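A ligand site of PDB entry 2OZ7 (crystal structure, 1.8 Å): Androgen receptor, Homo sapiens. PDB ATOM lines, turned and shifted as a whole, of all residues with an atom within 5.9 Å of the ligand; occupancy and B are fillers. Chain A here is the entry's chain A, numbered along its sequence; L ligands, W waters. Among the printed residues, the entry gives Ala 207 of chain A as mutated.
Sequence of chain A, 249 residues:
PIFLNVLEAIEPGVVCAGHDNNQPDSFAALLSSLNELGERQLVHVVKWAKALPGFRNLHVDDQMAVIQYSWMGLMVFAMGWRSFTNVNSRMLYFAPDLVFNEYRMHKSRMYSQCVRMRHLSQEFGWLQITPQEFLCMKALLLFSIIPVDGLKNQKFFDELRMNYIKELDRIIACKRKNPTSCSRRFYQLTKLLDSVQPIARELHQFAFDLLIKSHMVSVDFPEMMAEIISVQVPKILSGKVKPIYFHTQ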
ATOM      1  N   PHE A  27       6.149  -2.270 -14.973  1.00  0.00           N
ATOM      2  CA  PHE A  27       7.134  -1.890 -13.975  1.00  0.00           C
ATOM      3  C   PHE A  27       7.679  -0.508 -14.363  1.00  0.00           C
ATOM      4  O   PHE A  27       7.833   0.366 -13.522  1.00  0.00           O
ATOM      5  CB  PHE A  27       8.264  -2.918 -13.942  1.00  0.00           C
ATOM      6  CG  PHE A  27       9.391  -2.553 -13.031  1.00  0.00           C
ATOM      7  CD1 PHE A  27       9.158  -2.306 -11.684  1.00  0.00           C
ATOM      8  CD2 PHE A  27      10.686  -2.431 -13.517  1.00  0.00           C
ATOM      9  CE1 PHE A  27      10.203  -1.950 -10.827  1.00  0.00           C
ATOM     10  CE2 PHE A  27      11.741  -2.067 -12.676  1.00  0.00           C
ATOM     11  CZ  PHE A  27      11.503  -1.836 -11.328  1.00  0.00           C
ATOM     12  N   LEU A  31       7.393   2.827 -12.145  1.00  0.00           N
ATOM     13  CA  LEU A  31       8.685   3.324 -11.679  1.00  0.00           C
ATOM     14  C   LEU A  31       8.834   4.794 -12.047  1.00  0.00           C
ATOM     15  O   LEU A  31       9.194   5.623 -11.206  1.00  0.00           O
ATOM     16  CB  LEU A  31       9.815   2.510 -12.303  1.00  0.00           C
ATOM     17  CG  LEU A  31      11.233   3.010 -12.065  1.00  0.00           C
ATOM     18  CD1 LEU A  31      11.482   3.089 -10.572  1.00  0.00           C
ATOM     19  CD2 LEU A  31      12.256   2.067 -12.743  1.00  0.00           C
ATOM     20  N   SER A  33       6.582   6.979 -12.669  1.00  0.00           N
ATOM     21  CA  SER A  33       5.659   7.766 -11.868  1.00  0.00           C
ATOM     22  C   SER A  33       6.083   7.891 -10.411  1.00  0.00           C
ATOM     23  O   SER A  33       6.024   8.979  -9.848  1.00  0.00           O
ATOM     24  CB  SER A  33       4.253   7.168 -11.932  1.00  0.00           C
ATOM     25  OG  SER A  33       3.664   7.475 -13.183  1.00  0.00           O
ATOM     26  N   LEU A  34       6.497   6.774  -9.801  1.00  0.00           N
ATOM     27  CA  LEU A  34       6.932   6.823  -8.414  1.00  0.00           C
ATOM     28  C   LEU A  34       8.082   7.813  -8.246  1.00  0.00           C
ATOM     29  O   LEU A  34       8.049   8.682  -7.370  1.00  0.00           O
ATOM     30  CB  LEU A  34       7.381   5.437  -7.931  1.00  0.00           C
ATOM     31  CG  LEU A  34       6.274   4.435  -7.619  1.00  0.00           C
ATOM     32  CD1 LEU A  34       6.845   3.041  -7.449  1.00  0.00           C
ATOM     33  CD2 LEU A  34       5.544   4.873  -6.353  1.00  0.00           C
ATOM     34  N   ASN A  35       9.093   7.697  -9.102  1.00  0.00           N
ATOM     35  CA  ASN A  35      10.245   8.592  -9.044  1.00  0.00           C
ATOM     36  C   ASN A  35       9.870  10.050  -9.267  1.00  0.00           C
ATOM     37  O   ASN A  35      10.371  10.942  -8.588  1.00  0.00           O
ATOM     38  CB  ASN A  35      11.298   8.176 -10.077  1.00  0.00           C
ATOM     39  CG  ASN A  35      12.048   6.933  -9.656  1.00  0.00           C
ATOM     40  OD1 ASN A  35      12.756   6.321 -10.463  1.00  0.00           O
ATOM     41  ND2 ASN A  35      11.907   6.563  -8.398  1.00  0.00           N
ATOM     42  N   LEU A  37       7.031  11.401  -8.639  1.00  0.00           N
ATOM     43  CA  LEU A  37       6.354  11.806  -7.421  1.00  0.00           C
ATOM     44  C   LEU A  37       7.391  12.033  -6.315  1.00  0.00           C
ATOM     45  O   LEU A  37       7.290  12.993  -5.550  1.00  0.00           O
ATOM     46  CB  LEU A  37       5.352  10.728  -6.981  1.00  0.00           C
ATOM     47  CG  LEU A  37       4.589  11.002  -5.690  1.00  0.00           C
ATOM     48  CD1 LEU A  37       3.891  12.359  -5.766  1.00  0.00           C
ATOM     49  CD2 LEU A  37       3.595   9.888  -5.442  1.00  0.00           C
ATOM     50  N   GLY A  38       8.380  11.148  -6.258  1.00  0.00           N
ATOM     51  CA  GLY A  38       9.422  11.257  -5.247  1.00  0.00           C
ATOM     52  C   GLY A  38      10.166  12.578  -5.327  1.00  0.00           C
ATOM     53  O   GLY A  38      10.335  13.267  -4.316  1.00  0.00           O
ATOM     54  N   GLN A  41       7.865  15.539  -4.326  1.00  0.00           N
ATOM     55  CA  GLN A  41       7.670  15.635  -2.891  1.00  0.00           C
ATOM     56  C   GLN A  41       8.897  16.172  -2.177  1.00  0.00           C
ATOM     57  O   GLN A  41       8.802  17.019  -1.286  1.00  0.00           O
ATOM     58  CB  GLN A  41       7.320  14.268  -2.327  1.00  0.00           C
ATOM     59  CG  GLN A  41       5.914  13.830  -2.641  1.00  0.00           C
ATOM     60  CD  GLN A  41       5.684  12.398  -2.265  1.00  0.00           C
ATOM     61  OE1 GLN A  41       4.544  11.944  -2.145  1.00  0.00           O
ATOM     62  NE2 GLN A  41       6.775  11.674  -2.077  1.00  0.00           N
ATOM     63  N   TRP A  71      14.326  11.195   4.824  1.00  0.00           N
ATOM     64  CA  TRP A  71      13.463  11.291   3.656  1.00  0.00           C
ATOM     65  C   TRP A  71      12.527  10.099   3.466  1.00  0.00           C
ATOM     66  O   TRP A  71      11.304  10.237   3.541  1.00  0.00           O
ATOM     67  CB  TRP A  71      14.308  11.491   2.398  1.00  0.00           C
ATOM     68  CG  TRP A  71      13.558  11.300   1.117  1.00  0.00           C
ATOM     69  CD1 TRP A  71      12.479  12.019   0.678  1.00  0.00           C
ATOM     70  CD2 TRP A  71      13.822  10.324   0.098  1.00  0.00           C
ATOM     71  NE1 TRP A  71      12.058  11.548  -0.543  1.00  0.00           N
ATOM     72  CE2 TRP A  71      12.868  10.508  -0.928  1.00  0.00           C
ATOM     73  CE3 TRP A  71      14.781   9.311  -0.042  1.00  0.00           C
ATOM     74  CZ2 TRP A  71      12.844   9.719  -2.079  1.00  0.00           C
ATOM     75  CZ3 TRP A  71      14.752   8.519  -1.185  1.00  0.00           C
ATOM     76  CH2 TRP A  71      13.788   8.732  -2.191  1.00  0.00           C
ATOM     77  N   MET A  72      13.095   8.920   3.221  1.00  0.00           N
ATOM     78  CA  MET A  72      12.300   7.724   2.987  1.00  0.00           C
ATOM     79  C   MET A  72      11.284   7.425   4.090  1.00  0.00           C
ATOM     80  O   MET A  72      10.115   7.178   3.813  1.00  0.00           O
ATOM     81  CB  MET A  72      13.204   6.510   2.776  1.00  0.00           C
ATOM     82  CG  MET A  72      12.467   5.268   2.274  1.00  0.00           C
ATOM     83  SD  MET A  72      11.851   5.434   0.591  1.00  0.00           S
ATOM     84  CE  MET A  72      13.404   5.328  -0.298  1.00  0.00           C
ATOM     85  N   MET A  75       8.373   9.769   3.962  1.00  0.00           N
ATOM     86  CA  MET A  75       7.440   9.494   2.883  1.00  0.00           C
ATOM     87  C   MET A  75       6.598   8.265   3.204  1.00  0.00           C
ATOM     88  O   MET A  75       5.406   8.229   2.891  1.00  0.00           O
ATOM     89  CB  MET A  75       8.184   9.295   1.555  1.00  0.00           C
ATOM     90  CG  MET A  75       8.921  10.538   1.074  1.00  0.00           C
ATOM     91  SD  MET A  75       7.847  11.993   0.844  1.00  0.00           S
ATOM     92  CE  MET A  75       7.820  12.685   2.489  1.00  0.00           C
ATOM     93  N   VAL A  76       7.202   7.267   3.837  1.00  0.00           N
ATOM     94  CA  VAL A  76       6.458   6.073   4.210  1.00  0.00           C
ATOM     95  C   VAL A  76       5.351   6.464   5.171  1.00  0.00           C
ATOM     96  O   VAL A  76       4.183   6.154   4.939  1.00  0.00           O
ATOM     97  CB  VAL A  76       7.348   5.026   4.891  1.00  0.00           C
ATOM     98  CG1 VAL A  76       6.491   3.950   5.534  1.00  0.00           C
ATOM     99  CG2 VAL A  76       8.270   4.385   3.869  1.00  0.00           C
ATOM    100  N   MET A  79       2.680   8.810   3.570  1.00  0.00           N
ATOM    101  CA  MET A  79       1.926   8.026   2.600  1.00  0.00           C
ATOM    102  C   MET A  79       0.929   7.153   3.350  1.00  0.00           C
ATOM    103  O   MET A  79      -0.239   7.037   2.960  1.00  0.00           O
ATOM    104  CB  MET A  79       2.889   7.157   1.769  1.00  0.00           C
ATOM    105  CG  MET A  79       2.249   6.431   0.592  1.00  0.00           C
ATOM    106  SD  MET A  79       1.360   4.911   1.032  1.00  0.00           S
ATOM    107  CE  MET A  79       2.740   3.743   1.122  1.00  0.00           C
ATOM    108  N   ARG A  82      -2.052   9.183   4.398  1.00  0.00           N
ATOM    109  CA  ARG A  82      -2.945   9.505   3.287  1.00  0.00           C
ATOM    110  C   ARG A  82      -3.796   8.297   2.925  1.00  0.00           C
ATOM    111  O   ARG A  82      -4.970   8.439   2.559  1.00  0.00           O
ATOM    112  CB  ARG A  82      -2.153   9.954   2.046  1.00  0.00           C
ATOM    113  CG  ARG A  82      -1.508  11.328   2.175  1.00  0.00           C
ATOM    114  CD  ARG A  82      -1.035  11.854   0.815  1.00  0.00           C
ATOM    115  NE  ARG A  82      -0.027  10.999   0.185  1.00  0.00           N
ATOM    116  CZ  ARG A  82       1.272  11.018   0.466  1.00  0.00           C
ATOM    117  NH1 ARG A  82       1.743  11.866   1.372  1.00  0.00           N
ATOM    118  NH2 ARG A  82       2.110  10.209  -0.169  1.00  0.00           N
ATOM    119  N   PHE A  94      -0.337   6.752  -2.779  1.00  0.00           N
ATOM    120  CA  PHE A  94       0.890   7.513  -2.972  1.00  0.00           C
ATOM    121  C   PHE A  94       0.523   8.922  -3.394  1.00  0.00           C
ATOM    122  O   PHE A  94       1.163   9.893  -3.011  1.00  0.00           O
ATOM    123  CB  PHE A  94       1.771   6.881  -4.040  1.00  0.00           C
ATOM    124  CG  PHE A  94       2.402   5.585  -3.618  1.00  0.00           C
ATOM    125  CD1 PHE A  94       1.837   4.367  -3.976  1.00  0.00           C
ATOM    126  CD2 PHE A  94       3.575   5.590  -2.859  1.00  0.00           C
ATOM    127  CE1 PHE A  94       2.420   3.162  -3.588  1.00  0.00           C
ATOM    128  CE2 PHE A  94       4.160   4.385  -2.457  1.00  0.00           C
ATOM    129  CZ  PHE A  94       3.595   3.168  -2.816  1.00  0.00           C
ATOM    130  N   LEU A  98      -2.098   8.295  -8.206  1.00  0.00           N
ATOM    131  CA  LEU A  98      -1.261   7.107  -8.140  1.00  0.00           C
ATOM    132  C   LEU A  98      -1.617   6.298  -6.902  1.00  0.00           C
ATOM    133  O   LEU A  98      -0.961   6.402  -5.862  1.00  0.00           O
ATOM    134  CB  LEU A  98       0.215   7.497  -8.138  1.00  0.00           C
ATOM    135  CG  LEU A  98       1.218   6.340  -8.234  1.00  0.00           C
ATOM    136  CD1 LEU A  98       0.973   5.579  -9.533  1.00  0.00           C
ATOM    137  CD2 LEU A  98       2.640   6.877  -8.205  1.00  0.00           C
ATOM    138  N   SER A 108       5.016  -3.374  -9.154  1.00  0.00           N
ATOM    139  CA  SER A 108       6.101  -2.506  -8.717  1.00  0.00           C
ATOM    140  C   SER A 108       7.320  -3.308  -8.248  1.00  0.00           C
ATOM    141  O   SER A 108       8.437  -2.790  -8.197  1.00  0.00           O
ATOM    142  CB  SER A 108       5.633  -1.613  -7.572  1.00  0.00           C
ATOM    143  OG  SER A 108       5.370  -2.386  -6.425  1.00  0.00           O
ATOM    144  N   ARG A 109       7.080  -4.570  -7.907  1.00  0.00           N
ATOM    145  CA  ARG A 109       8.139  -5.481  -7.451  1.00  0.00           C
ATOM    146  C   ARG A 109       8.529  -5.244  -5.996  1.00  0.00           C
ATOM    147  O   ARG A 109       9.545  -5.747  -5.538  1.00  0.00           O
ATOM    148  CB  ARG A 109       9.357  -5.375  -8.362  1.00  0.00           C
ATOM    149  CG  ARG A 109       9.057  -5.784  -9.784  1.00  0.00           C
ATOM    150  CD  ARG A 109      10.211  -5.539 -10.715  1.00  0.00           C
ATOM    151  NE  ARG A 109       9.921  -6.018 -12.064  1.00  0.00           N
ATOM    152  CZ  ARG A 109      10.726  -5.831 -13.111  1.00  0.00           C
ATOM    153  NH1 ARG A 109      11.866  -5.174 -12.976  1.00  0.00           N
ATOM    154  NH2 ARG A 109      10.386  -6.305 -14.297  1.00  0.00           N
ATOM    155  N   MET A 110       7.702  -4.493  -5.281  1.00  0.00           N
ATOM    156  CA  MET A 110       7.941  -4.205  -3.868  1.00  0.00           C
ATOM    157  C   MET A 110       6.721  -4.671  -3.076  1.00  0.00           C
ATOM    158  O   MET A 110       6.344  -4.043  -2.072  1.00  0.00           O
ATOM    159  CB  MET A 110       8.078  -2.705  -3.617  1.00  0.00           C
ATOM    160  CG  MET A 110       8.801  -1.903  -4.646  1.00  0.00           C
ATOM    161  SD  MET A 110       8.850  -0.235  -3.993  1.00  0.00           S
ATOM    162  CE  MET A 110      10.286  -0.356  -2.960  1.00  0.00           C
ATOM    163  N   MET A 117       3.700  -1.651   4.492  1.00  0.00           N
ATOM    164  CA  MET A 117       3.267  -0.262   4.556  1.00  0.00           C
ATOM    165  C   MET A 117       1.754  -0.212   4.766  1.00  0.00           C
ATOM    166  O   MET A 117       1.235   0.699   5.417  1.00  0.00           O
ATOM    167  CB  MET A 117       3.679   0.503   3.293  1.00  0.00           C
ATOM    168  CG  MET A 117       5.188   0.721   3.177  1.00  0.00           C
ATOM    169  SD  MET A 117       5.672   1.977   1.962  1.00  0.00           S
ATOM    170  CE  MET A 117       5.702   1.005   0.471  1.00  0.00           C
ATOM    171  N   LEU A 203      13.176  -0.281   1.919  1.00  0.00           N
ATOM    172  CA  LEU A 203      12.965   0.597   0.777  1.00  0.00           C
ATOM    173  C   LEU A 203      14.276   1.242   0.373  1.00  0.00           C
ATOM    174  O   LEU A 203      14.517   1.547  -0.793  1.00  0.00           O
ATOM    175  CB  LEU A 203      11.934   1.660   1.116  1.00  0.00           C
ATOM    176  CG  LEU A 203      10.557   1.081   1.411  1.00  0.00           C
ATOM    177  CD1 LEU A 203       9.592   2.181   1.783  1.00  0.00           C
ATOM    178  CD2 LEU A 203      10.056   0.349   0.175  1.00  0.00           C
ATOM    179  N   PHE A 206      16.132  -1.455  -1.558  1.00  0.00           N
ATOM    180  CA  PHE A 206      15.491  -1.613  -2.847  1.00  0.00           C
ATOM    181  C   PHE A 206      15.876  -0.468  -3.782  1.00  0.00           C
ATOM    182  O   PHE A 206      16.245  -0.694  -4.946  1.00  0.00           O
ATOM    183  CB  PHE A 206      13.975  -1.665  -2.638  1.00  0.00           C
ATOM    184  CG  PHE A 206      13.235  -2.319  -3.765  1.00  0.00           C
ATOM    185  CD1 PHE A 206      13.052  -1.656  -4.971  1.00  0.00           C
ATOM    186  CD2 PHE A 206      12.736  -3.607  -3.608  1.00  0.00           C
ATOM    187  CE1 PHE A 206      12.372  -2.281  -6.020  1.00  0.00           C
ATOM    188  CE2 PHE A 206      12.051  -4.223  -4.643  1.00  0.00           C
ATOM    189  CZ  PHE A 206      11.867  -3.560  -5.863  1.00  0.00           C
ATOM    190  N   ALA A 207      15.826   0.754  -3.262  1.00  0.00           N
ATOM    191  CA  ALA A 207      16.191   1.916  -4.061  1.00  0.00           C
ATOM    192  C   ALA A 207      17.640   1.877  -4.521  1.00  0.00           C
ATOM    193  O   ALA A 207      17.941   2.139  -5.685  1.00  0.00           O
ATOM    194  CB  ALA A 207      15.933   3.195  -3.257  1.00  0.00           C
ATOM    195  N   PHE A 208      18.534   1.552  -3.603  1.00  0.00           N
ATOM    196  CA  PHE A 208      19.955   1.473  -3.908  1.00  0.00           C
ATOM    197  C   PHE A 208      20.171   0.463  -5.012  1.00  0.00           C
ATOM    198  O   PHE A 208      20.758   0.785  -6.047  1.00  0.00           O
ATOM    199  CB  PHE A 208      20.750   1.059  -2.661  1.00  0.00           C
ATOM    200  CG  PHE A 208      22.204   0.890  -2.917  1.00  0.00           C
ATOM    201  CD1 PHE A 208      23.024   1.996  -3.109  1.00  0.00           C
ATOM    202  CD2 PHE A 208      22.763  -0.377  -3.008  1.00  0.00           C
ATOM    203  CE1 PHE A 208      24.387   1.847  -3.383  1.00  0.00           C
ATOM    204  CE2 PHE A 208      24.127  -0.550  -3.281  1.00  0.00           C
ATOM    205  CZ  PHE A 208      24.935   0.572  -3.473  1.00  0.00           C
ATOM    206  N   LEU A 210      18.169  -0.778  -7.217  1.00  0.00           N
ATOM    207  CA  LEU A 210      17.604  -0.352  -8.483  1.00  0.00           C
ATOM    208  C   LEU A 210      18.466   0.716  -9.141  1.00  0.00           C
ATOM    209  O   LEU A 210      18.703   0.655 -10.341  1.00  0.00           O
ATOM    210  CB  LEU A 210      16.176   0.164  -8.268  1.00  0.00           C
ATOM    211  CG  LEU A 210      15.257   0.157  -9.496  1.00  0.00           C
ATOM    212  CD1 LEU A 210      15.195  -1.247 -10.088  1.00  0.00           C
ATOM    213  CD2 LEU A 210      13.870   0.609  -9.097  1.00  0.00           C
ATOM    214  N   LEU A 211      18.943   1.674  -8.355  1.00  0.00           N
ATOM    215  CA  LEU A 211      19.788   2.738  -8.897  1.00  0.00           C
ATOM    216  C   LEU A 211      21.019   2.179  -9.587  1.00  0.00           C
ATOM    217  O   LEU A 211      21.411   2.657 -10.650  1.00  0.00           O
ATOM    218  CB  LEU A 211      20.240   3.688  -7.773  1.00  0.00           C
ATOM    219  CG  LEU A 211      21.221   4.776  -8.246  1.00  0.00           C
ATOM    220  CD1 LEU A 211      20.518   5.678  -9.255  1.00  0.00           C
ATOM    221  CD2 LEU A 211      21.719   5.584  -7.063  1.00  0.00           C
ATOM    222  N   PHE A 221      16.840   8.140 -13.084  1.00  0.00           N
ATOM    223  CA  PHE A 221      16.501   8.506 -11.716  1.00  0.00           C
ATOM    224  C   PHE A 221      16.660  10.015 -11.575  1.00  0.00           C
ATOM    225  O   PHE A 221      17.707  10.558 -11.924  1.00  0.00           O
ATOM    226  CB  PHE A 221      17.434   7.818 -10.715  1.00  0.00           C
ATOM    227  CG  PHE A 221      16.874   6.554 -10.124  1.00  0.00           C
ATOM    228  CD1 PHE A 221      16.658   5.430 -10.911  1.00  0.00           C
ATOM    229  CD2 PHE A 221      16.589   6.484  -8.764  1.00  0.00           C
ATOM    230  CE1 PHE A 221      16.167   4.245 -10.353  1.00  0.00           C
ATOM    231  CE2 PHE A 221      16.093   5.308  -8.192  1.00  0.00           C
ATOM    232  CZ  PHE A 221      15.893   4.184  -8.995  1.00  0.00           C
ATOM    233  N   MET A 225      16.760  12.643  -6.021  1.00  0.00           N
ATOM    234  CA  MET A 225      16.652  11.263  -5.569  1.00  0.00           C
ATOM    235  C   MET A 225      17.990  10.566  -5.816  1.00  0.00           C
ATOM    236  O   MET A 225      18.505   9.869  -4.959  1.00  0.00           O
ATOM    237  CB  MET A 225      15.542  10.528  -6.337  1.00  0.00           C
ATOM    238  CG  MET A 225      14.134  10.899  -5.889  1.00  0.00           C
ATOM    239  SD  MET A 225      12.885   9.884  -6.678  1.00  0.00           S
ATOM    240  CE  MET A 225      13.543   8.224  -6.371  1.00  0.00           C
ATOM    241  N   ILE A 229      20.300   8.736  -2.901  1.00  0.00           N
ATOM    242  CA  ILE A 229      20.505   7.301  -2.988  1.00  0.00           C
ATOM    243  C   ILE A 229      21.969   6.900  -3.212  1.00  0.00           C
ATOM    244  O   ILE A 229      22.431   5.898  -2.656  1.00  0.00           O
ATOM    245  CB  ILE A 229      19.596   6.706  -4.098  1.00  0.00           C
ATOM    246  CG1 ILE A 229      18.124   6.893  -3.692  1.00  0.00           C
ATOM    247  CG2 ILE A 229      19.898   5.224  -4.314  1.00  0.00           C
ATOM    248  CD1 ILE A 229      17.130   6.522  -4.767  1.00  0.00           C
HETATM  249  C1  LIG L   1       6.415   7.264  -1.288  1.00  0.00           C
HETATM  250  C2  LIG L   1      10.353   3.978  -3.634  1.00  0.00           C
HETATM  251  C3  LIG L   1       7.514   6.573  -1.794  1.00  0.00           C
HETATM  252  C4  LIG L   1       7.958   5.440  -1.123  1.00  0.00           C
HETATM  253  C5  LIG L   1       9.819   6.535  -4.893  1.00  0.00           C
HETATM  254  C6  LIG L   1       9.076   4.723  -1.565  1.00  0.00           C
HETATM  255  C7  LIG L   1       9.876   5.164  -2.793  1.00  0.00           C
HETATM  256  C8  LIG L   1       9.006   6.047  -3.697  1.00  0.00           C
HETATM  257  C9  LIG L   1       8.418   7.188  -2.870  1.00  0.00           C
HETATM  258  C10 LIG L   1      10.339   5.355  -5.717  1.00  0.00           C
HETATM  259  C11 LIG L   1      11.185   4.455  -4.824  1.00  0.00           C
HETATM  260  C12 LIG L   1       5.882   8.380  -1.920  1.00  0.00           C
HETATM  261  C13 LIG L   1       9.519   7.942  -2.124  1.00  0.00           C
HETATM  262  C14 LIG L   1       7.712   8.196  -3.777  1.00  0.00           C
HETATM  263  C15 LIG L   1       6.332   7.839  -4.354  1.00  0.00           C
HETATM  264  C16 LIG L   1       6.454   8.891  -3.240  1.00  0.00           C
HETATM  265  O1  LIG L   1       4.945   8.980  -1.400  1.00  0.00           O
HETATM  266 CL1  LIG L   1       7.132   4.932   0.311  1.00  0.00          CL
HETATM  267  C17 LIG L   1      12.440   5.187  -4.364  1.00  0.00           C
HETATM  268  C18 LIG L   1      11.316   2.999  -2.964  1.00  0.00           C
HETATM  269  C19 LIG L   1      11.998   2.320  -4.164  1.00  0.00           C
HETATM  270  C20 LIG L   1      11.518   3.073  -5.405  1.00  0.00           C
HETATM  271  C21 LIG L   1      12.601   3.171  -6.492  1.00  0.00           C
HETATM  272  C22 LIG L   1      14.063   2.959  -6.113  1.00  0.00           C
HETATM  273  O2  LIG L   1      12.286   3.381  -7.663  1.00  0.00           O
HETATM  274  O3  LIG L   1      10.306   2.489  -5.904  1.00  0.00           O
HETATM  275  C23 LIG L   1      10.484   1.266  -6.474  1.00  0.00           C
HETATM  276  C24 LIG L   1       9.281   0.554  -7.083  1.00  0.00           C
HETATM  277  O4  LIG L   1      11.597   0.741  -6.504  1.00  0.00           O
HETATM  278  O   HOH W   1       4.586  10.452   1.123  1.00  0.00           O
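Water W1 lies within hydrogen-bond range of NH2 of Arg 82 (2.8 Å), O1 of the ligand (2.9 Å) and O of Met 75 (3.0 Å).
The side-chain hydroxyl of Ser 108 lies close to the backbone NH of Met 110, at 3.3 Å.
NE2 of Gln 41 sits at hydrogen-bond distance from SD of Met 75, at 3.1 Å.
The guanidinium group (NH2) of Arg 82 sits at hydrogen-bond distance from the backbone carbonyl oxygen (O) of Phe 94 (3.0 Å).
The side-chain sulfur (SD) of Met 110 sits close to an oxygen (O3) of the ligand (3.6 Å).
Merely in contact with the ligand: Leu 31, Ala 207, Phe 206, Leu 210, Leu 34, Met 72, Leu 37, Ser 108, Phe 221, Phe 94, Met 117, Trp 71, Val 76, Gly 38, Met 225, Met 75 and Leu 203.
Hydrophobic or aromatic side chains that line the ligand: Leu 31, Leu 34, Leu 37, Trp 71, Met 72, Met 75, Val 76, Phe 94, Met 110, Met 117, Leu 203, Phe 206, Ala 207, Leu 210, Phe 221 and Met 225.
Within 4 Å of the ligand: Leu 31, Leu 34, Asn 35, Leu 37, Gly 38, Gln 41, Trp 71, Met 72, Met 75, Val 76, Arg 82, Phe 94, Ser 108, Met 110, Met 117, Leu 203, Phe 206, Ala 207, Leu 210, Phe 221 and Met 225.
The guanidinium group of Arg 82 lies within hydrogen-bond range of an oxygen (O1) of the ligand (3.3 Å).
The side-chain amide nitrogen (ND2) of Asn 35 sits at hydrogen-bond distance from an oxygen (O2) of the ligand (3.3 Å).
An oxygen (O1) of the ligand sits close to the side-chain amide oxygen of Gln 41 (3.1 Å).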
